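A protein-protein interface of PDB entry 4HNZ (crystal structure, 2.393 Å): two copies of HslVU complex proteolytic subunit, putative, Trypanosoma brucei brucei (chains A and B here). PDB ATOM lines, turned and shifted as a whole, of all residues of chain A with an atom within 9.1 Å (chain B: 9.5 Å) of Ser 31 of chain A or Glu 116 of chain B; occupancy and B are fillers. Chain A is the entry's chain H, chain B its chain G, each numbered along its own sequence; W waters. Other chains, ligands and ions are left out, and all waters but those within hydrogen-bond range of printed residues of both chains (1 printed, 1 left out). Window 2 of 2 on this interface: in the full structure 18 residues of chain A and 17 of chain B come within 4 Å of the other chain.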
ATOM      1  N   GLY A  16      20.087  23.343 -29.311  1.00  0.00           N
ATOM      2  CA  GLY A  16      19.202  22.246 -29.139  1.00  0.00           C
ATOM      3  C   GLY A  16      18.976  21.864 -27.685  1.00  0.00           C
ATOM      4  O   GLY A  16      19.868  22.004 -26.868  1.00  0.00           O
ATOM      5  N   ASP A  17      17.787  21.336 -27.389  1.00  0.00           N
ATOM      6  CA  ASP A  17      17.506  20.873 -26.029  1.00  0.00           C
ATOM      7  C   ASP A  17      18.054  19.480 -25.845  1.00  0.00           C
ATOM      8  O   ASP A  17      18.749  18.958 -26.744  1.00  0.00           O
ATOM      9  CB  ASP A  17      16.036  20.907 -25.705  1.00  0.00           C
ATOM     10  CG  ASP A  17      15.303  19.669 -26.189  1.00  0.00           C
ATOM     11  OD1 ASP A  17      15.328  19.454 -27.420  1.00  0.00           O
ATOM     12  OD2 ASP A  17      14.773  18.935 -25.320  1.00  0.00           O
ATOM     13  N   ARG A  18      17.868  18.917 -24.656  1.00  0.00           N
ATOM     14  CA  ARG A  18      18.600  17.689 -24.288  1.00  0.00           C
ATOM     15  C   ARG A  18      17.697  16.573 -23.814  1.00  0.00           C
ATOM     16  O   ARG A  18      18.172  15.600 -23.255  1.00  0.00           O
ATOM     17  CB  ARG A  18      19.709  17.993 -23.273  1.00  0.00           C
ATOM     18  CG  ARG A  18      20.715  19.114 -23.660  1.00  0.00           C
ATOM     19  CD  ARG A  18      21.780  19.460 -22.552  1.00  0.00           C
ATOM     20  NE  ARG A  18      23.005  18.858 -22.977  1.00  0.00           N
ATOM     21  CZ  ARG A  18      23.810  18.067 -22.286  1.00  0.00           C
ATOM     22  NH1 ARG A  18      23.653  17.824 -20.993  1.00  0.00           N
ATOM     23  NH2 ARG A  18      24.842  17.548 -22.915  1.00  0.00           N
ATOM     24  N   GLN A  19      16.378  16.731 -24.000  1.00  0.00           N
ATOM     25  CA  GLN A  19      15.409  15.759 -23.491  1.00  0.00           C
ATOM     26  C   GLN A  19      15.203  14.619 -24.470  1.00  0.00           C
ATOM     27  O   GLN A  19      14.923  14.867 -25.623  1.00  0.00           O
ATOM     28  CB  GLN A  19      14.068  16.409 -23.221  1.00  0.00           C
ATOM     29  CG  GLN A  19      13.036  15.455 -22.580  1.00  0.00           C
ATOM     30  CD  GLN A  19      11.767  16.194 -22.111  1.00  0.00           C
ATOM     31  OE1 GLN A  19      11.881  17.156 -21.448  1.00  0.00           O
ATOM     32  NE2 GLN A  19      10.595  15.805 -22.601  1.00  0.00           N
ATOM     33  N   VAL A  20      15.329  13.391 -24.028  1.00  0.00           N
ATOM     34  CA  VAL A  20      14.846  12.287 -24.831  1.00  0.00           C
ATOM     35  C   VAL A  20      13.603  11.695 -24.195  1.00  0.00           C
ATOM     36  O   VAL A  20      13.600  11.299 -23.043  1.00  0.00           O
ATOM     37  CB  VAL A  20      15.924  11.175 -24.987  1.00  0.00           C
ATOM     38  CG1 VAL A  20      15.386  10.019 -25.822  1.00  0.00           C
ATOM     39  CG2 VAL A  20      17.176  11.747 -25.640  1.00  0.00           C
ATOM     40  N   VAL A  27      10.435  10.965 -19.847  1.00  0.00           N
ATOM     41  CA  VAL A  27      11.793  11.405 -20.077  1.00  0.00           C
ATOM     42  C   VAL A  27      12.678  10.215 -19.721  1.00  0.00           C
ATOM     43  O   VAL A  27      12.711   9.786 -18.600  1.00  0.00           O
ATOM     44  CB  VAL A  27      12.158  12.620 -19.186  1.00  0.00           C
ATOM     45  CG1 VAL A  27      13.634  12.990 -19.357  1.00  0.00           C
ATOM     46  CG2 VAL A  27      11.235  13.763 -19.485  1.00  0.00           C
ATOM     47  N   ALA A  28      13.363   9.670 -20.706  1.00  0.00           N
ATOM     48  CA  ALA A  28      14.372   8.629 -20.500  1.00  0.00           C
ATOM     49  C   ALA A  28      15.774   9.210 -20.277  1.00  0.00           C
ATOM     50  O   ALA A  28      16.617   8.567 -19.627  1.00  0.00           O
ATOM     51  CB  ALA A  28      14.411   7.699 -21.666  1.00  0.00           C
ATOM     52  N   LYS A  29      15.999  10.435 -20.742  1.00  0.00           N
ATOM     53  CA  LYS A  29      17.293  11.121 -20.539  1.00  0.00           C
ATOM     54  C   LYS A  29      17.069  12.614 -20.610  1.00  0.00           C
ATOM     55  O   LYS A  29      16.339  13.077 -21.478  1.00  0.00           O
ATOM     56  CB  LYS A  29      18.297  10.702 -21.633  1.00  0.00           C
ATOM     57  CG  LYS A  29      19.721  11.200 -21.405  1.00  0.00           C
ATOM     58  CD  LYS A  29      20.749  10.424 -22.237  1.00  0.00           C
ATOM     59  CE  LYS A  29      22.166  10.927 -22.044  1.00  0.00           C
ATOM     60  NZ  LYS A  29      22.652  10.646 -20.651  1.00  0.00           N
ATOM     61  N   SER A  30      17.711  13.361 -19.744  1.00  0.00           N
ATOM     62  CA  SER A  30      17.601  14.813 -19.770  1.00  0.00           C
ATOM     63  C   SER A  30      18.919  15.541 -20.195  1.00  0.00           C
ATOM     64  O   SER A  30      18.968  16.745 -20.146  1.00  0.00           O
ATOM     65  CB  SER A  30      17.110  15.324 -18.399  1.00  0.00           C
ATOM     66  OG  SER A  30      18.072  15.029 -17.435  1.00  0.00           O
ATOM     67  N   SER A  31      19.952  14.789 -20.580  1.00  0.00           N
ATOM     68  CA  SER A  31      21.243  15.333 -20.870  1.00  0.00           C
ATOM     69  C   SER A  31      21.772  14.801 -22.187  1.00  0.00           C
ATOM     70  O   SER A  31      22.963  14.597 -22.327  1.00  0.00           O
ATOM     71  CB  SER A  31      22.192  14.950 -19.769  1.00  0.00           C
ATOM     72  OG  SER A  31      22.198  13.539 -19.625  1.00  0.00           O
ATOM     73  N   ALA A  32      20.924  14.602 -23.186  1.00  0.00           N
ATOM     74  CA  ALA A  32      21.377  14.103 -24.489  1.00  0.00           C
ATOM     75  C   ALA A  32      21.805  15.276 -25.389  1.00  0.00           C
ATOM     76  O   ALA A  32      21.052  16.231 -25.534  1.00  0.00           O
ATOM     77  CB  ALA A  32      20.238  13.333 -25.168  1.00  0.00           C
ATOM     78  N   CYS A  33      22.901  15.141 -26.114  1.00  0.00           N
ATOM     79  CA  CYS A  33      23.351  16.177 -27.020  1.00  0.00           C
ATOM     80  C   CYS A  33      22.784  15.944 -28.417  1.00  0.00           C
ATOM     81  O   CYS A  33      22.853  14.862 -28.945  1.00  0.00           O
ATOM     82  CB  CYS A  33      24.887  16.247 -27.056  1.00  0.00           C
ATOM     83  SG  CYS A  33      25.415  17.744 -27.964  1.00  0.00           S
ATOM     84  N   LYS A  34      22.180  16.970 -29.000  1.00  0.00           N
ATOM     85  CA  LYS A  34      21.509  16.824 -30.279  1.00  0.00           C
ATOM     86  C   LYS A  34      22.182  17.595 -31.383  1.00  0.00           C
ATOM     87  O   LYS A  34      21.629  17.715 -32.481  1.00  0.00           O
ATOM     88  CB  LYS A  34      20.020  17.266 -30.151  1.00  0.00           C
ATOM     89  CG  LYS A  34      19.246  16.422 -29.192  1.00  0.00           C
ATOM     90  CD  LYS A  34      17.819  16.892 -29.000  1.00  0.00           C
ATOM     91  CE  LYS A  34      17.111  16.132 -27.887  1.00  0.00           C
ATOM     92  NZ  LYS A  34      15.822  16.732 -27.556  1.00  0.00           N
ATOM     93  N   ARG A  36      25.920  18.193 -33.615  1.00  0.00           N
ATOM     94  CA  ARG A  36      27.177  17.604 -33.975  1.00  0.00           C
ATOM     95  C   ARG A  36      27.956  18.590 -34.831  1.00  0.00           C
ATOM     96  O   ARG A  36      27.390  19.313 -35.643  1.00  0.00           O
ATOM     97  CB  ARG A  36      27.005  16.300 -34.728  1.00  0.00           C
ATOM     98  CG  ARG A  36      26.394  15.167 -33.927  1.00  0.00           C
ATOM     99  CD  ARG A  36      27.281  14.627 -32.803  1.00  0.00           C
ATOM    100  NE  ARG A  36      26.649  13.449 -32.179  1.00  0.00           N
ATOM    101  CZ  ARG A  36      25.648  13.482 -31.284  1.00  0.00           C
ATOM    102  NH1 ARG A  36      25.133  14.641 -30.850  1.00  0.00           N
ATOM    103  NH2 ARG A  36      25.146  12.353 -30.824  1.00  0.00           N
ATOM    104  N   ASN A 164      13.292  20.191 -22.948  1.00  0.00           N
ATOM    105  CA  ASN A 164      13.667  20.636 -21.566  1.00  0.00           C
ATOM    106  C   ASN A 164      14.457  21.905 -21.594  1.00  0.00           C
ATOM    107  O   ASN A 164      14.727  22.483 -22.654  1.00  0.00           O
ATOM    108  CB  ASN A 164      14.347  19.514 -20.738  1.00  0.00           C
ATOM    109  CG  ASN A 164      15.724  19.136 -21.250  1.00  0.00           C
ATOM    110  OD1 ASN A 164      16.312  19.815 -22.132  1.00  0.00           O
ATOM    111  ND2 ASN A 164      16.245  18.049 -20.741  1.00  0.00           N
ATOM    112  N   GLU A 165      14.897  22.302 -20.430  1.00  0.00           N
ATOM    113  CA  GLU A 165      15.522  23.622 -20.230  1.00  0.00           C
ATOM    114  C   GLU A 165      17.025  23.613 -20.371  1.00  0.00           C
ATOM    115  O   GLU A 165      17.644  24.607 -20.125  1.00  0.00           O
ATOM    116  CB  GLU A 165      15.139  24.163 -18.856  1.00  0.00           C
ATOM    117  CG  GLU A 165      15.813  23.479 -17.670  1.00  0.00           C
ATOM    118  CD  GLU A 165      15.051  22.254 -17.109  1.00  0.00           C
ATOM    119  OE1 GLU A 165      14.316  21.535 -17.840  1.00  0.00           O
ATOM    120  OE2 GLU A 165      15.241  21.982 -15.877  1.00  0.00           O
ATOM    121  N   HIS A 166      17.613  22.483 -20.722  1.00  0.00           N
ATOM    122  CA  HIS A 166      19.079  22.386 -20.816  1.00  0.00           C
ATOM    123  C   HIS A 166      19.424  22.406 -22.305  1.00  0.00           C
ATOM    124  O   HIS A 166      18.849  21.664 -23.092  1.00  0.00           O
ATOM    125  CB  HIS A 166      19.577  21.124 -20.115  1.00  0.00           C
ATOM    126  CG  HIS A 166      19.199  21.026 -18.652  1.00  0.00           C
ATOM    127  ND1 HIS A 166      19.685  21.888 -17.693  1.00  0.00           N
ATOM    128  CD2 HIS A 166      18.408  20.140 -17.987  1.00  0.00           C
ATOM    129  CE1 HIS A 166      19.198  21.557 -16.510  1.00  0.00           C
ATOM    130  NE2 HIS A 166      18.408  20.507 -16.663  1.00  0.00           N
ATOM    131  N   TRP A 167      20.314  23.306 -22.717  1.00  0.00           N
ATOM    132  CA  TRP A 167      20.581  23.527 -24.138  1.00  0.00           C
ATOM    133  C   TRP A 167      22.035  23.414 -24.471  1.00  0.00           C
ATOM    134  O   TRP A 167      22.873  23.827 -23.728  1.00  0.00           O
ATOM    135  CB  TRP A 167      20.080  24.889 -24.582  1.00  0.00           C
ATOM    136  CG  TRP A 167      18.739  25.178 -24.055  1.00  0.00           C
ATOM    137  CD1 TRP A 167      17.643  24.360 -24.108  1.00  0.00           C
ATOM    138  CD2 TRP A 167      18.324  26.357 -23.380  1.00  0.00           C
ATOM    139  NE1 TRP A 167      16.580  24.962 -23.477  1.00  0.00           N
ATOM    140  CE2 TRP A 167      16.966  26.191 -23.037  1.00  0.00           C
ATOM    141  CE3 TRP A 167      18.954  27.557 -23.079  1.00  0.00           C
ATOM    142  CZ2 TRP A 167      16.223  27.183 -22.434  1.00  0.00           C
ATOM    143  CZ3 TRP A 167      18.222  28.543 -22.425  1.00  0.00           C
ATOM    144  CH2 TRP A 167      16.869  28.337 -22.117  1.00  0.00           C
ATOM    145  N   ASP A 168      22.327  22.868 -25.639  1.00  0.00           N
ATOM    146  CA  ASP A 168      23.655  22.941 -26.217  1.00  0.00           C
ATOM    147  C   ASP A 168      23.668  24.050 -27.260  1.00  0.00           C
ATOM    148  O   ASP A 168      22.655  24.304 -27.925  1.00  0.00           O
ATOM    149  CB  ASP A 168      24.032  21.594 -26.842  1.00  0.00           C
ATOM    150  CG  ASP A 168      24.311  20.542 -25.799  1.00  0.00           C
ATOM    151  OD1 ASP A 168      25.259  20.731 -25.046  1.00  0.00           O
ATOM    152  OD2 ASP A 168      23.587  19.530 -25.713  1.00  0.00           O
ATOM    153  N   SER B   5      19.362  -1.697 -14.187  1.00  0.00           N
ATOM    154  CA  SER B   5      20.801  -1.619 -13.899  1.00  0.00           C
ATOM    155  C   SER B   5      21.045  -0.446 -12.983  1.00  0.00           C
ATOM    156  O   SER B   5      20.561   0.657 -13.230  1.00  0.00           O
ATOM    157  CB  SER B   5      21.590  -1.409 -15.208  1.00  0.00           C
ATOM    158  OG  SER B   5      22.978  -1.271 -14.938  1.00  0.00           O
ATOM    159  N   VAL B   6      21.841  -0.642 -11.973  1.00  0.00           N
ATOM    160  CA  VAL B   6      22.246   0.433 -11.075  1.00  0.00           C
ATOM    161  C   VAL B   6      23.769   0.392 -10.893  1.00  0.00           C
ATOM    162  O   VAL B   6      24.325  -0.672 -10.553  1.00  0.00           O
ATOM    163  CB  VAL B   6      21.634   0.234  -9.670  1.00  0.00           C
ATOM    164  CG1 VAL B   6      22.064   1.350  -8.728  1.00  0.00           C
ATOM    165  CG2 VAL B   6      20.123   0.113  -9.752  1.00  0.00           C
ATOM    166  N   ARG B   7      24.420   1.521 -11.126  1.00  0.00           N
ATOM    167  CA  ARG B   7      25.833   1.667 -10.895  1.00  0.00           C
ATOM    168  C   ARG B   7      25.991   2.617  -9.724  1.00  0.00           C
ATOM    169  O   ARG B   7      25.484   3.711  -9.759  1.00  0.00           O
ATOM    170  CB  ARG B   7      26.537   2.250 -12.138  1.00  0.00           C
ATOM    171  CG  ARG B   7      28.040   2.539 -11.952  1.00  0.00           C
ATOM    172  CD  ARG B   7      28.748   3.009 -13.223  1.00  0.00           C
ATOM    173  NE  ARG B   7      28.974   1.889 -14.160  1.00  0.00           N
ATOM    174  CZ  ARG B   7      28.187   1.589 -15.210  1.00  0.00           C
ATOM    175  NH1 ARG B   7      27.109   2.345 -15.493  1.00  0.00           N
ATOM    176  NH2 ARG B   7      28.460   0.531 -15.986  1.00  0.00           N
ATOM    177  N   LYS B   8      26.632   2.154  -8.676  1.00  0.00           N
ATOM    178  CA  LYS B   8      27.007   3.021  -7.600  1.00  0.00           C
ATOM    179  C   LYS B   8      28.421   2.616  -7.086  1.00  0.00           C
ATOM    180  O   LYS B   8      28.649   1.459  -6.699  1.00  0.00           O
ATOM    181  CB  LYS B   8      25.981   2.937  -6.464  1.00  0.00           C
ATOM    182  CG  LYS B   8      26.320   3.859  -5.290  1.00  0.00           C
ATOM    183  CD  LYS B   8      25.268   3.717  -4.181  1.00  0.00           C
ATOM    184  CE  LYS B   8      25.413   4.743  -3.089  1.00  0.00           C
ATOM    185  NZ  LYS B   8      24.151   4.864  -2.319  1.00  0.00           N
ATOM    186  N   THR B 103      27.206   1.660 -19.231  1.00  0.00           N
ATOM    187  CA  THR B 103      25.883   1.074 -19.418  1.00  0.00           C
ATOM    188  C   THR B 103      25.141   1.793 -20.534  1.00  0.00           C
ATOM    189  O   THR B 103      25.043   3.004 -20.523  1.00  0.00           O
ATOM    190  CB  THR B 103      24.999   1.162 -18.125  1.00  0.00           C
ATOM    191  OG1 THR B 103      25.720   0.616 -17.016  1.00  0.00           O
ATOM    192  CG2 THR B 103      23.721   0.401 -18.287  1.00  0.00           C
ATOM    193  N   GLU B 105      21.465   1.569 -23.005  1.00  0.00           N
ATOM    194  CA  GLU B 105      20.182   1.050 -23.324  1.00  0.00           C
ATOM    195  C   GLU B 105      19.982   1.284 -24.806  1.00  0.00           C
ATOM    196  O   GLU B 105      20.251   2.399 -25.324  1.00  0.00           O
ATOM    197  CB  GLU B 105      19.142   1.755 -22.452  1.00  0.00           C
ATOM    198  CG  GLU B 105      17.725   1.746 -22.983  1.00  0.00           C
ATOM    199  CD  GLU B 105      16.763   2.600 -22.161  1.00  0.00           C
ATOM    200  OE1 GLU B 105      17.141   3.099 -21.089  1.00  0.00           O
ATOM    201  OE2 GLU B 105      15.601   2.794 -22.627  1.00  0.00           O
ATOM    202  N   VAL B 112      19.838   5.274 -28.111  1.00  0.00           N
ATOM    203  CA  VAL B 112      20.930   4.719 -27.377  1.00  0.00           C
ATOM    204  C   VAL B 112      21.051   5.645 -26.154  1.00  0.00           C
ATOM    205  O   VAL B 112      21.413   6.763 -26.307  1.00  0.00           O
ATOM    206  CB  VAL B 112      22.210   4.744 -28.202  1.00  0.00           C
ATOM    207  CG1 VAL B 112      23.371   4.196 -27.401  1.00  0.00           C
ATOM    208  CG2 VAL B 112      22.029   3.917 -29.453  1.00  0.00           C
ATOM    209  N   ILE B 113      20.738   5.142 -24.971  1.00  0.00           N
ATOM    210  CA  ILE B 113      20.568   5.964 -23.798  1.00  0.00           C
ATOM    211  C   ILE B 113      21.565   5.492 -22.787  1.00  0.00           C
ATOM    212  O   ILE B 113      21.657   4.308 -22.521  1.00  0.00           O
ATOM    213  CB  ILE B 113      19.163   5.816 -23.257  1.00  0.00           C
ATOM    214  CG1 ILE B 113      18.207   6.612 -24.154  1.00  0.00           C
ATOM    215  CG2 ILE B 113      19.053   6.240 -21.797  1.00  0.00           C
ATOM    216  CD1 ILE B 113      16.845   5.976 -24.247  1.00  0.00           C
ATOM    217  N   THR B 114      22.400   6.429 -22.337  1.00  0.00           N
ATOM    218  CA  THR B 114      23.293   6.225 -21.236  1.00  0.00           C
ATOM    219  C   THR B 114      22.638   6.908 -20.022  1.00  0.00           C
ATOM    220  O   THR B 114      21.828   7.817 -20.162  1.00  0.00           O
ATOM    221  CB  THR B 114      24.638   6.899 -21.489  1.00  0.00           C
ATOM    222  OG1 THR B 114      24.395   8.282 -21.763  1.00  0.00           O
ATOM    223  CG2 THR B 114      25.345   6.286 -22.707  1.00  0.00           C
ATOM    224  N   PRO B 115      23.020   6.491 -18.811  1.00  0.00           N
ATOM    225  CA  PRO B 115      22.353   6.982 -17.615  1.00  0.00           C
ATOM    226  C   PRO B 115      22.759   8.407 -17.323  1.00  0.00           C
ATOM    227  O   PRO B 115      23.725   8.895 -17.873  1.00  0.00           O
ATOM    228  CB  PRO B 115      22.886   6.068 -16.516  1.00  0.00           C
ATOM    229  CG  PRO B 115      24.163   5.531 -17.050  1.00  0.00           C
ATOM    230  CD  PRO B 115      24.004   5.427 -18.534  1.00  0.00           C
ATOM    231  N   GLU B 116      22.015   9.057 -16.439  1.00  0.00           N
ATOM    232  CA  GLU B 116      22.467  10.295 -15.827  1.00  0.00           C
ATOM    233  C   GLU B 116      23.578   9.982 -14.803  1.00  0.00           C
ATOM    234  O   GLU B 116      24.012   8.858 -14.661  1.00  0.00           O
ATOM    235  CB  GLU B 116      21.305  11.016 -15.106  1.00  0.00           C
ATOM    236  CG  GLU B 116      19.980  11.175 -15.889  1.00  0.00           C
ATOM    237  CD  GLU B 116      20.112  11.944 -17.209  1.00  0.00           C
ATOM    238  OE1 GLU B 116      21.091  12.688 -17.427  1.00  0.00           O
ATOM    239  OE2 GLU B 116      19.261  11.774 -18.082  1.00  0.00           O
ATOM    240  N   ALA B 117      24.006  10.978 -14.070  1.00  0.00           N
ATOM    241  CA  ALA B 117      25.008  10.769 -13.102  1.00  0.00           C
ATOM    242  C   ALA B 117      24.585   9.741 -12.069  1.00  0.00           C
ATOM    243  O   ALA B 117      25.441   9.136 -11.409  1.00  0.00           O
ATOM    244  CB  ALA B 117      25.390  12.124 -12.426  1.00  0.00           C
ATOM    245  N   ASP B 118      23.307   9.525 -11.878  1.00  0.00           N
ATOM    246  CA  ASP B 118      22.887   8.583 -10.860  1.00  0.00           C
ATOM    247  C   ASP B 118      23.153   7.142 -11.240  1.00  0.00           C
ATOM    248  O   ASP B 118      22.907   6.225 -10.450  1.00  0.00           O
ATOM    249  CB  ASP B 118      21.403   8.802 -10.526  1.00  0.00           C
ATOM    250  CG  ASP B 118      20.495   8.533 -11.727  1.00  0.00           C
ATOM    251  OD1 ASP B 118      20.867   7.768 -12.673  1.00  0.00           O
ATOM    252  OD2 ASP B 118      19.375   9.072 -11.706  1.00  0.00           O
ATOM    253  N   GLY B 119      23.646   6.881 -12.440  1.00  0.00           N
ATOM    254  CA  GLY B 119      23.996   5.475 -12.826  1.00  0.00           C
ATOM    255  C   GLY B 119      22.826   4.502 -13.087  1.00  0.00           C
ATOM    256  O   GLY B 119      23.038   3.269 -13.183  1.00  0.00           O
ATOM    257  N   ILE B 120      21.608   5.006 -13.263  1.00  0.00           N
ATOM    258  CA  ILE B 120      20.431   4.119 -13.386  1.00  0.00           C
ATOM    259  C   ILE B 120      19.847   4.087 -14.779  1.00  0.00           C
ATOM    260  O   ILE B 120      19.596   5.111 -15.402  1.00  0.00           O
ATOM    261  CB  ILE B 120      19.338   4.563 -12.416  1.00  0.00           C
ATOM    262  CG1 ILE B 120      19.843   4.400 -10.983  1.00  0.00           C
ATOM    263  CG2 ILE B 120      18.060   3.786 -12.624  1.00  0.00           C
ATOM    264  CD1 ILE B 120      18.996   5.196 -10.009  1.00  0.00           C
ATOM    265  N   VAL B 121      19.646   2.882 -15.270  1.00  0.00           N
ATOM    266  CA  VAL B 121      19.008   2.623 -16.566  1.00  0.00           C
ATOM    267  C   VAL B 121      17.990   1.488 -16.371  1.00  0.00           C
ATOM    268  O   VAL B 121      18.285   0.540 -15.671  1.00  0.00           O
ATOM    269  CB  VAL B 121      20.068   2.132 -17.599  1.00  0.00           C
ATOM    270  CG1 VAL B 121      19.441   1.780 -18.930  1.00  0.00           C
ATOM    271  CG2 VAL B 121      21.089   3.201 -17.828  1.00  0.00           C
ATOM    272  N   ALA B 122      16.851   1.553 -17.055  1.00  0.00           N
ATOM    273  CA  ALA B 122      15.865   0.497 -16.991  1.00  0.00           C
ATOM    274  C   ALA B 122      14.981   0.416 -18.215  1.00  0.00           C
ATOM    275  O   ALA B 122      14.761   1.421 -18.876  1.00  0.00           O
ATOM    276  CB  ALA B 122      15.011   0.701 -15.781  1.00  0.00           C
ATOM    277  N   LYS B 131      13.131   2.394 -12.076  1.00  0.00           N
ATOM    278  CA  LYS B 131      13.936   3.517 -12.090  1.00  0.00           C
ATOM    279  C   LYS B 131      13.529   4.532 -11.053  1.00  0.00           C
ATOM    280  O   LYS B 131      14.405   5.154 -10.406  1.00  0.00           O
ATOM    281  CB  LYS B 131      13.866   4.099 -13.502  1.00  0.00           C
ATOM    282  CG  LYS B 131      14.584   5.407 -13.635  1.00  0.00           C
ATOM    283  CD  LYS B 131      14.291   5.997 -14.988  1.00  0.00           C
ATOM    284  CE  LYS B 131      15.449   5.748 -15.930  1.00  0.00           C
ATOM    285  NZ  LYS B 131      15.216   6.607 -17.141  1.00  0.00           N
ATOM    286  N   ARG B 135      15.959   5.635  -8.095  1.00  0.00           N
ATOM    287  CA  ARG B 135      16.366   7.061  -7.947  1.00  0.00           C
ATOM    288  C   ARG B 135      16.077   7.634  -6.580  1.00  0.00           C
ATOM    289  O   ARG B 135      16.838   8.479  -6.102  1.00  0.00           O
ATOM    290  CB  ARG B 135      15.716   7.957  -8.972  1.00  0.00           C
ATOM    291  CG  ARG B 135      16.398   7.850 -10.282  1.00  0.00           C
ATOM    292  CD  ARG B 135      15.886   8.866 -11.285  1.00  0.00           C
ATOM    293  NE  ARG B 135      16.691   8.808 -12.505  1.00  0.00           N
ATOM    294  CZ  ARG B 135      16.303   9.248 -13.676  1.00  0.00           C
ATOM    295  NH1 ARG B 135      15.086   9.755 -13.850  1.00  0.00           N
ATOM    296  NH2 ARG B 135      17.150   9.165 -14.722  1.00  0.00           N
ATOM    297  N   ILE B 138      19.205   6.157  -4.550  1.00  0.00           N
ATOM    298  CA  ILE B 138      20.568   6.114  -5.109  1.00  0.00           C
ATOM    299  C   ILE B 138      21.572   6.846  -4.208  1.00  0.00           C
ATOM    300  O   ILE B 138      22.740   6.419  -4.044  1.00  0.00           O
ATOM    301  CB  ILE B 138      20.598   6.674  -6.541  1.00  0.00           C
ATOM    302  CG1 ILE B 138      21.968   6.416  -7.234  1.00  0.00           C
ATOM    303  CG2 ILE B 138      20.261   8.186  -6.577  1.00  0.00           C
ATOM    304  CD1 ILE B 138      22.337   4.940  -7.403  1.00  0.00           C
HETATM  305  O   HOH W   1      19.471   8.370 -18.664  1.00  0.00           O
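O of Thr 114 of chain B is in hydrogen-bond range of NZ of Lys 29 of chain A (3.0 Å). The backbone carbonyl oxygen (O) of Pro 115 of chain B lies within hydrogen-bond range of the side-chain amino group (NZ) of Lys 29 of chain A, at 3.5 Å. N of Ser 30 of chain A sits at hydrogen-bond distance from OE2 of Glu 116 of chain B, 2.8 Å away. The side-chain hydroxyl (OG) of Ser 31 of chain A lies within hydrogen-bond range of the side-chain carboxylate (OE1) of Glu 116 of chain B, 2.6 Å away. The backbone carbonyl oxygen (O) of Ala 28 of chain A lies within hydrogen-bond range of the side-chain amino group (NZ) of Lys 131 of chain B.
O of Ile 113 of chain B sits at hydrogen-bond distance from N of Glu 105 of chain B (2.8 Å). The backbone NH (N) of Ser 31 of chain A sits at hydrogen-bond distance from the backbone carbonyl oxygen (O) of Arg 18 of chain A, 3.3 Å away. The backbone carbonyl oxygen of Val 20 of chain A sits at hydrogen-bond distance from the backbone NH of Ala 28 of chain A (2.9 Å). The backbone carbonyl oxygen of Lys 29 of chain A is in hydrogen-bond range of the backbone NH of Val 20 of chain A, at 2.8 Å. The side-chain hydroxyl of Ser 31 of chain A lies within hydrogen-bond range of the side-chain amino group of Lys 29 of chain A (3.1 Å). The backbone carbonyl oxygen (O) of Ser 30 of chain A is in hydrogen-bond range of the side-chain amide nitrogen (ND2) of Asn 164 of chain A.
Among the printed residues, merely in contact across the chains: Ala 28 of chain A with Ile 113 of chain B (3.9 Å) and Lys 29 of chain A with Glu 116 of chain B (3.2 Å).
Ser 31 of chain A touches just one residue of chain B: Glu 116 (2.6 Å). Glu 116 of chain B touches just these residues of chain A: Lys 29, Ser 30 and Ser 31. Printed residues of chain B within 4 Å of Lys 29 of chain A: Thr 114, Pro 115 and Glu 116. Printed residues of chain B within 4 Å of Ser 30 of chain A: Glu 116 (2.8 Å). No residue of chain B comes within 4 Å of Ala 32 of chain A. Of chain A, only Lys 29 comes within 4 Å of Pro 115 of chain B. Of the printed residues of chain A, Thr 114 of chain B touches Lys 29 (3.0 Å). Printed residues of chain B within 4 Å of Ala 28 of chain A: Ile 113 and Lys 131. Printed residues of chain A within 4 Å of Lys 131 of chain B: Ala 28. Printed residues of chain A within 4 Å of Ile 113 of chain B: Ala 28. Glu 105 of chain B touches none of the printed residues of chain A. The nearest residue of chain B that does not touch Ser 31 of chain A is Pro 115 of chain B (5.2 Å). The nearest printed residue of chain A that does not touch Ile 113 of chain B is Lys 29 of chain A (4.5 Å).
Hydrophobic or aromatic side chains of chain A within 4 Å of the printed part of chain B: Ala 28. Printed residues of chain B that touch a printed residue of chain A: Ile 113, Thr 114, Pro 115, Glu 116 and Lys 131. Hydrophobic or aromatic side chains of chain B that line the printed part of chain A: Ile 113. Among the printed residues, 7 pairs touch across the chains.
No position is printed for both chains. Of the 7 pairs that touch across the chains among the printed residues, none has its exchanged pair printed and touching as well.
Water W1 lies within hydrogen-bond range of O of Thr 114 of chain B, O of Ala 28 of chain A and N of Glu 116 of chain B.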
